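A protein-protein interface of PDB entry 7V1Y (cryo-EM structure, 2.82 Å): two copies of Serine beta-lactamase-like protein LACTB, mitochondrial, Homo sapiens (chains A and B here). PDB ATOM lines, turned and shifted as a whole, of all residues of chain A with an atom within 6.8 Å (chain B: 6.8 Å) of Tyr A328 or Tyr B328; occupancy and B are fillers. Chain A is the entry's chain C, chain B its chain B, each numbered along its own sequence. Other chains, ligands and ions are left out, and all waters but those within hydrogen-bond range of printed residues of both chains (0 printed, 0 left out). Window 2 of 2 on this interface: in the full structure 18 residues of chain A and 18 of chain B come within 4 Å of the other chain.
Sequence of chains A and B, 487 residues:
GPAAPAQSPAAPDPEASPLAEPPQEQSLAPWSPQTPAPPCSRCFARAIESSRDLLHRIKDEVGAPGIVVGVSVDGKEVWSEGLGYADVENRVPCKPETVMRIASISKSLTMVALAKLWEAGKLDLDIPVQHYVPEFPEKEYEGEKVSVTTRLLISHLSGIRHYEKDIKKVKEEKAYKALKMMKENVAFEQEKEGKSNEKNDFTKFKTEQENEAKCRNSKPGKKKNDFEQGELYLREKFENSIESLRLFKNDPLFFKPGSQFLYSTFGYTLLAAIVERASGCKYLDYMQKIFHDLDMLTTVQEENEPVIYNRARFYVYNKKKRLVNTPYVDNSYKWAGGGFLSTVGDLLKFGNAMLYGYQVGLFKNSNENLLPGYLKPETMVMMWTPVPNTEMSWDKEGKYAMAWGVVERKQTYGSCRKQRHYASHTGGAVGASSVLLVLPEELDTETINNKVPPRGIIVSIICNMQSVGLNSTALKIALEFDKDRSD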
ATOM      1  N   ARG A 101      25.915  16.456  21.494  1.00  0.00           N
ATOM      2  CA  ARG A 101      24.505  16.256  21.841  1.00  0.00           C
ATOM      3  C   ARG A 101      24.098  16.564  23.256  1.00  0.00           C
ATOM      4  O   ARG A 101      24.269  15.724  24.137  1.00  0.00           O
ATOM      5  CB  ARG A 101      24.118  14.793  21.609  1.00  0.00           C
ATOM      6  CG  ARG A 101      23.871  14.370  20.178  1.00  0.00           C
ATOM      7  CD  ARG A 101      23.646  12.871  20.127  1.00  0.00           C
ATOM      8  NE  ARG A 101      23.486  12.376  18.765  1.00  0.00           N
ATOM      9  CZ  ARG A 101      23.425  11.089  18.443  1.00  0.00           C
ATOM     10  NH1 ARG A 101      23.517  10.164  19.388  1.00  0.00           N
ATOM     11  NH2 ARG A 101      23.279  10.727  17.178  1.00  0.00           N
ATOM     12  N   TYR A 233      16.699   3.226  20.665  1.00  0.00           N
ATOM     13  CA  TYR A 233      17.485   3.028  19.454  1.00  0.00           C
ATOM     14  C   TYR A 233      16.597   3.020  18.218  1.00  0.00           C
ATOM     15  O   TYR A 233      16.843   2.289  17.256  1.00  0.00           O
ATOM     16  CB  TYR A 233      18.300   1.740  19.541  1.00  0.00           C
ATOM     17  CG  TYR A 233      19.368   1.768  20.610  1.00  0.00           C
ATOM     18  CD1 TYR A 233      20.600   2.358  20.369  1.00  0.00           C
ATOM     19  CD2 TYR A 233      19.141   1.209  21.858  1.00  0.00           C
ATOM     20  CE1 TYR A 233      21.577   2.388  21.343  1.00  0.00           C
ATOM     21  CE2 TYR A 233      20.111   1.236  22.838  1.00  0.00           C
ATOM     22  CZ  TYR A 233      21.328   1.825  22.574  1.00  0.00           C
ATOM     23  OH  TYR A 233      22.299   1.854  23.547  1.00  0.00           O
ATOM     24  N   LEU A 234      15.546   3.834  18.229  1.00  0.00           N
ATOM     25  CA  LEU A 234      14.660   3.932  17.079  1.00  0.00           C
ATOM     26  C   LEU A 234      15.334   4.691  15.942  1.00  0.00           C
ATOM     27  O   LEU A 234      16.224   5.519  16.155  1.00  0.00           O
ATOM     28  CB  LEU A 234      13.355   4.625  17.465  1.00  0.00           C
ATOM     29  CG  LEU A 234      12.314   3.775  18.198  1.00  0.00           C
ATOM     30  CD1 LEU A 234      10.972   4.485  18.222  1.00  0.00           C
ATOM     31  CD2 LEU A 234      12.188   2.405  17.553  1.00  0.00           C
ATOM     32  N   ARG A 235      14.900   4.396  14.715  1.00  0.00           N
ATOM     33  CA  ARG A 235      15.432   5.052  13.529  1.00  0.00           C
ATOM     34  C   ARG A 235      14.356   5.636  12.626  1.00  0.00           C
ATOM     35  O   ARG A 235      14.691   6.201  11.580  1.00  0.00           O
ATOM     36  CB  ARG A 235      16.293   4.074  12.716  1.00  0.00           C
ATOM     37  CG  ARG A 235      17.553   3.621  13.428  1.00  0.00           C
ATOM     38  CD  ARG A 235      18.362   2.675  12.559  1.00  0.00           C
ATOM     39  NE  ARG A 235      17.604   1.482  12.204  1.00  0.00           N
ATOM     40  CZ  ARG A 235      18.150   0.320  11.875  1.00  0.00           C
ATOM     41  NH1 ARG A 235      19.463   0.158  11.844  1.00  0.00           N
ATOM     42  NH2 ARG A 235      17.360  -0.705  11.570  1.00  0.00           N
ATOM     43  N   ASN A 304      20.384  14.316  10.111  1.00  0.00           N
ATOM     44  CA  ASN A 304      21.473  13.692   9.371  1.00  0.00           C
ATOM     45  C   ASN A 304      21.722  14.331   8.012  1.00  0.00           C
ATOM     46  O   ASN A 304      22.879  14.541   7.637  1.00  0.00           O
ATOM     47  CB  ASN A 304      21.190  12.197   9.185  1.00  0.00           C
ATOM     48  CG  ASN A 304      22.246  11.503   8.350  1.00  0.00           C
ATOM     49  OD1 ASN A 304      21.967  11.021   7.252  1.00  0.00           O
ATOM     50  ND2 ASN A 304      23.466  11.446   8.867  1.00  0.00           N
ATOM     51  N   THR A 326      28.881   4.249  18.368  1.00  0.00           N
ATOM     52  CA  THR A 326      27.509   4.016  18.786  1.00  0.00           C
ATOM     53  C   THR A 326      26.617   3.779  17.568  1.00  0.00           C
ATOM     54  O   THR A 326      26.889   4.299  16.482  1.00  0.00           O
ATOM     55  CB  THR A 326      26.982   5.204  19.586  1.00  0.00           C
ATOM     56  OG1 THR A 326      27.372   6.424  18.950  1.00  0.00           O
ATOM     57  CG2 THR A 326      27.532   5.177  21.000  1.00  0.00           C
ATOM     58  N   PRO A 327      25.555   2.993  17.719  1.00  0.00           N
ATOM     59  CA  PRO A 327      24.660   2.740  16.585  1.00  0.00           C
ATOM     60  C   PRO A 327      23.918   3.995  16.154  1.00  0.00           C
ATOM     61  O   PRO A 327      23.698   4.921  16.940  1.00  0.00           O
ATOM     62  CB  PRO A 327      23.690   1.680  17.122  1.00  0.00           C
ATOM     63  CG  PRO A 327      23.784   1.785  18.604  1.00  0.00           C
ATOM     64  CD  PRO A 327      25.188   2.196  18.900  1.00  0.00           C
ATOM     65  N   TYR A 328      23.539   4.018  14.878  1.00  0.00           N
ATOM     66  CA  TYR A 328      22.813   5.154  14.326  1.00  0.00           C
ATOM     67  C   TYR A 328      21.397   5.198  14.888  1.00  0.00           C
ATOM     68  O   TYR A 328      20.700   4.179  14.926  1.00  0.00           O
ATOM     69  CB  TYR A 328      22.783   5.064  12.800  1.00  0.00           C
ATOM     70  CG  TYR A 328      21.785   5.987  12.138  1.00  0.00           C
ATOM     71  CD1 TYR A 328      22.082   7.327  11.934  1.00  0.00           C
ATOM     72  CD2 TYR A 328      20.551   5.516  11.707  1.00  0.00           C
ATOM     73  CE1 TYR A 328      21.176   8.173  11.327  1.00  0.00           C
ATOM     74  CE2 TYR A 328      19.640   6.355  11.097  1.00  0.00           C
ATOM     75  CZ  TYR A 328      19.957   7.682  10.911  1.00  0.00           C
ATOM     76  OH  TYR A 328      19.052   8.522  10.305  1.00  0.00           O
ATOM     77  N   VAL A 329      20.972   6.383  15.331  1.00  0.00           N
ATOM     78  CA  VAL A 329      19.653   6.576  15.921  1.00  0.00           C
ATOM     79  C   VAL A 329      19.021   7.833  15.341  1.00  0.00           C
ATOM     80  O   VAL A 329      19.703   8.725  14.832  1.00  0.00           O
ATOM     81  CB  VAL A 329      19.707   6.678  17.463  1.00  0.00           C
ATOM     82  CG1 VAL A 329      20.131   5.352  18.073  1.00  0.00           C
ATOM     83  CG2 VAL A 329      20.645   7.795  17.890  1.00  0.00           C
ATOM     84  N   ASP A 330      17.694   7.891  15.425  1.00  0.00           N
ATOM     85  CA  ASP A 330      16.920   9.060  15.029  1.00  0.00           C
ATOM     86  C   ASP A 330      16.139   9.559  16.235  1.00  0.00           C
ATOM     87  O   ASP A 330      15.418   8.787  16.875  1.00  0.00           O
ATOM     88  CB  ASP A 330      15.970   8.731  13.874  1.00  0.00           C
ATOM     89  CG  ASP A 330      15.484   9.971  13.147  1.00  0.00           C
ATOM     90  OD1 ASP A 330      15.818  11.092  13.584  1.00  0.00           O
ATOM     91  OD2 ASP A 330      14.766   9.823  12.137  1.00  0.00           O
ATOM     92  N   ARG B 101      34.351   4.084  -0.498  1.00  0.00           N
ATOM     93  CA  ARG B 101      33.587   2.900  -0.904  1.00  0.00           C
ATOM     94  C   ARG B 101      33.747   2.438  -2.327  1.00  0.00           C
ATOM     95  O   ARG B 101      33.090   2.970  -3.219  1.00  0.00           O
ATOM     96  CB  ARG B 101      32.090   3.161  -0.721  1.00  0.00           C
ATOM     97  CG  ARG B 101      31.551   3.078   0.690  1.00  0.00           C
ATOM     98  CD  ARG B 101      30.094   3.506   0.698  1.00  0.00           C
ATOM     99  NE  ARG B 101      29.529   3.535   2.042  1.00  0.00           N
ATOM    100  CZ  ARG B 101      28.325   4.015   2.331  1.00  0.00           C
ATOM    101  NH1 ARG B 101      27.559   4.514   1.371  1.00  0.00           N
ATOM    102  NH2 ARG B 101      27.887   4.002   3.583  1.00  0.00           N
ATOM    103  N   TYR B 233      18.448   1.299  -0.329  1.00  0.00           N
ATOM    104  CA  TYR B 233      18.555   2.063   0.908  1.00  0.00           C
ATOM    105  C   TYR B 233      18.128   1.229   2.108  1.00  0.00           C
ATOM    106  O   TYR B 233      17.534   1.736   3.062  1.00  0.00           O
ATOM    107  CB  TYR B 233      17.734   3.347   0.824  1.00  0.00           C
ATOM    108  CG  TYR B 233      18.249   4.330  -0.201  1.00  0.00           C
ATOM    109  CD1 TYR B 233      19.294   5.192   0.100  1.00  0.00           C
ATOM    110  CD2 TYR B 233      17.694   4.393  -1.471  1.00  0.00           C
ATOM    111  CE1 TYR B 233      19.770   6.089  -0.834  1.00  0.00           C
ATOM    112  CE2 TYR B 233      18.162   5.287  -2.410  1.00  0.00           C
ATOM    113  CZ  TYR B 233      19.200   6.134  -2.087  1.00  0.00           C
ATOM    114  OH  TYR B 233      19.671   7.027  -3.019  1.00  0.00           O
ATOM    115  N   LEU B 234      18.424  -0.066   2.074  1.00  0.00           N
ATOM    116  CA  LEU B 234      18.097  -0.940   3.190  1.00  0.00           C
ATOM    117  C   LEU B 234      19.027  -0.680   4.369  1.00  0.00           C
ATOM    118  O   LEU B 234      20.159  -0.218   4.209  1.00  0.00           O
ATOM    119  CB  LEU B 234      18.189  -2.406   2.768  1.00  0.00           C
ATOM    120  CG  LEU B 234      17.008  -2.971   1.976  1.00  0.00           C
ATOM    121  CD1 LEU B 234      17.086  -4.485   1.916  1.00  0.00           C
ATOM    122  CD2 LEU B 234      15.690  -2.523   2.585  1.00  0.00           C
ATOM    123  N   ARG B 235      18.531  -0.981   5.571  1.00  0.00           N
ATOM    124  CA  ARG B 235      19.305  -0.807   6.791  1.00  0.00           C
ATOM    125  C   ARG B 235      19.348  -2.052   7.664  1.00  0.00           C
ATOM    126  O   ARG B 235      19.962  -2.014   8.735  1.00  0.00           O
ATOM    127  CB  ARG B 235      18.751   0.366   7.615  1.00  0.00           C
ATOM    128  CG  ARG B 235      18.898   1.716   6.944  1.00  0.00           C
ATOM    129  CD  ARG B 235      18.350   2.826   7.822  1.00  0.00           C
ATOM    130  NE  ARG B 235      16.937   2.635   8.120  1.00  0.00           N
ATOM    131  CZ  ARG B 235      16.102   3.611   8.445  1.00  0.00           C
ATOM    132  NH1 ARG B 235      16.506   4.868   8.522  1.00  0.00           N
ATOM    133  NH2 ARG B 235      14.829   3.321   8.694  1.00  0.00           N
ATOM    134  N   ASN B 304      29.660  -0.321  10.609  1.00  0.00           N
ATOM    135  CA  ASN B 304      29.527   0.911  11.376  1.00  0.00           C
ATOM    136  C   ASN B 304      30.160   0.830  12.758  1.00  0.00           C
ATOM    137  O   ASN B 304      30.824   1.780  13.183  1.00  0.00           O
ATOM    138  CB  ASN B 304      28.046   1.280  11.518  1.00  0.00           C
ATOM    139  CG  ASN B 304      27.830   2.509  12.378  1.00  0.00           C
ATOM    140  OD1 ASN B 304      27.235   2.431  13.453  1.00  0.00           O
ATOM    141  ND2 ASN B 304      28.312   3.652  11.907  1.00  0.00           N
ATOM    142  N   THR B 326      24.422  11.844   2.466  1.00  0.00           N
ATOM    143  CA  THR B 326      23.649  10.711   1.989  1.00  0.00           C
ATOM    144  C   THR B 326      23.013   9.971   3.166  1.00  0.00           C
ATOM    145  O   THR B 326      23.558   9.970   4.274  1.00  0.00           O
ATOM    146  CB  THR B 326      24.532   9.753   1.196  1.00  0.00           C
ATOM    147  OG1 THR B 326      25.780   9.574   1.876  1.00  0.00           O
ATOM    148  CG2 THR B 326      24.792  10.300  -0.195  1.00  0.00           C
ATOM    149  N   PRO B 327      21.859   9.344   2.956  1.00  0.00           N
ATOM    150  CA  PRO B 327      21.211   8.610   4.048  1.00  0.00           C
ATOM    151  C   PRO B 327      22.020   7.397   4.478  1.00  0.00           C
ATOM    152  O   PRO B 327      22.795   6.827   3.705  1.00  0.00           O
ATOM    153  CB  PRO B 327      19.862   8.194   3.450  1.00  0.00           C
ATOM    154  CG  PRO B 327      20.051   8.273   1.976  1.00  0.00           C
ATOM    155  CD  PRO B 327      21.025   9.380   1.744  1.00  0.00           C
ATOM    156  N   TYR B 328      21.833   7.011   5.738  1.00  0.00           N
ATOM    157  CA  TYR B 328      22.536   5.859   6.287  1.00  0.00           C
ATOM    158  C   TYR B 328      22.001   4.573   5.671  1.00  0.00           C
ATOM    159  O   TYR B 328      20.786   4.373   5.582  1.00  0.00           O
ATOM    160  CB  TYR B 328      22.385   5.830   7.808  1.00  0.00           C
ATOM    161  CG  TYR B 328      22.778   4.520   8.451  1.00  0.00           C
ATOM    162  CD1 TYR B 328      24.110   4.217   8.696  1.00  0.00           C
ATOM    163  CD2 TYR B 328      21.815   3.589   8.824  1.00  0.00           C
ATOM    164  CE1 TYR B 328      24.472   3.023   9.287  1.00  0.00           C
ATOM    165  CE2 TYR B 328      22.170   2.394   9.415  1.00  0.00           C
ATOM    166  CZ  TYR B 328      23.498   2.115   9.643  1.00  0.00           C
ATOM    167  OH  TYR B 328      23.855   0.925  10.232  1.00  0.00           O
ATOM    168  N   VAL B 329      22.911   3.699   5.239  1.00  0.00           N
ATOM    169  CA  VAL B 329      22.553   2.438   4.601  1.00  0.00           C
ATOM    170  C   VAL B 329      23.405   1.319   5.184  1.00  0.00           C
ATOM    171  O   VAL B 329      24.482   1.546   5.740  1.00  0.00           O
ATOM    172  CB  VAL B 329      22.726   2.483   3.066  1.00  0.00           C
ATOM    173  CG1 VAL B 329      21.724   3.443   2.443  1.00  0.00           C
ATOM    174  CG2 VAL B 329      24.148   2.873   2.701  1.00  0.00           C
ATOM    175  N   ASP B 330      22.902   0.093   5.050  1.00  0.00           N
ATOM    176  CA  ASP B 330      23.620  -1.111   5.441  1.00  0.00           C
ATOM    177  C   ASP B 330      23.787  -1.998   4.218  1.00  0.00           C
ATOM    178  O   ASP B 330      22.808  -2.309   3.533  1.00  0.00           O
ATOM    179  CB  ASP B 330      22.879  -1.863   6.551  1.00  0.00           C
ATOM    180  CG  ASP B 330      23.771  -2.847   7.285  1.00  0.00           C
ATOM    181  OD1 ASP B 330      24.943  -3.005   6.887  1.00  0.00           O
ATOM    182  OD2 ASP B 330      23.298  -3.461   8.264  1.00  0.00           O
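Among the printed residues, merely in contact across the chains: Asn A304 with Thr B326, Thr A326 with Asn B304, Tyr A328 with Tyr B328 and Arg A235 with Arg B235.
Of the printed residues of chain B, Asn A304 touches Thr B326 (3.5 Å).
Of the printed residues of chain B, Thr A326 touches Asn B304 (3.6 Å).
Tyr A328 touches one residue of chain B.
Arg B101 touches none of the printed residues of chain A.
Leu B234 touches none of the printed residues of chain A.
Of the printed residues of chain A, Arg B235 touches Arg A235 (3.8 Å).
Of chain A, only Tyr A328 comes within 4 Å of Tyr B328.
The nearest printed residue of chain A that does not touch Tyr B328 is Arg A235 (4.3 Å).
Of the 10 printed residues of chain B, 4 touch a printed residue of chain A.
Printed residues of chain B that touch a printed residue of chain A: Arg B235, Asn B304, Thr B326 and Tyr B328.
Hydrophobic or aromatic side chains of chain B within 4 Å of the printed part of chain A: Tyr B328.
Printed residues of chain A that touch a printed residue of chain B: Arg A235, Asn A304, Thr A326 and Tyr A328.
Hydrophobic or aromatic side chains of chain A within 4 Å of the printed part of chain B: Tyr A328.
Arg A235 touches its own counterpart, Arg B235.
Asn A304 touches Thr B326, and with the chains exchanged Thr A326 touches Asn B304.
Tyr A328 touches its own counterpart, Tyr B328.
Positions printed for both chains: 101, 233, 234, 235, 304, 326, 327, 328, 329 and 330.
Of the 4 pairs that touch across the chains among the printed residues, 4 have their exchanged pair printed and touching as well.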
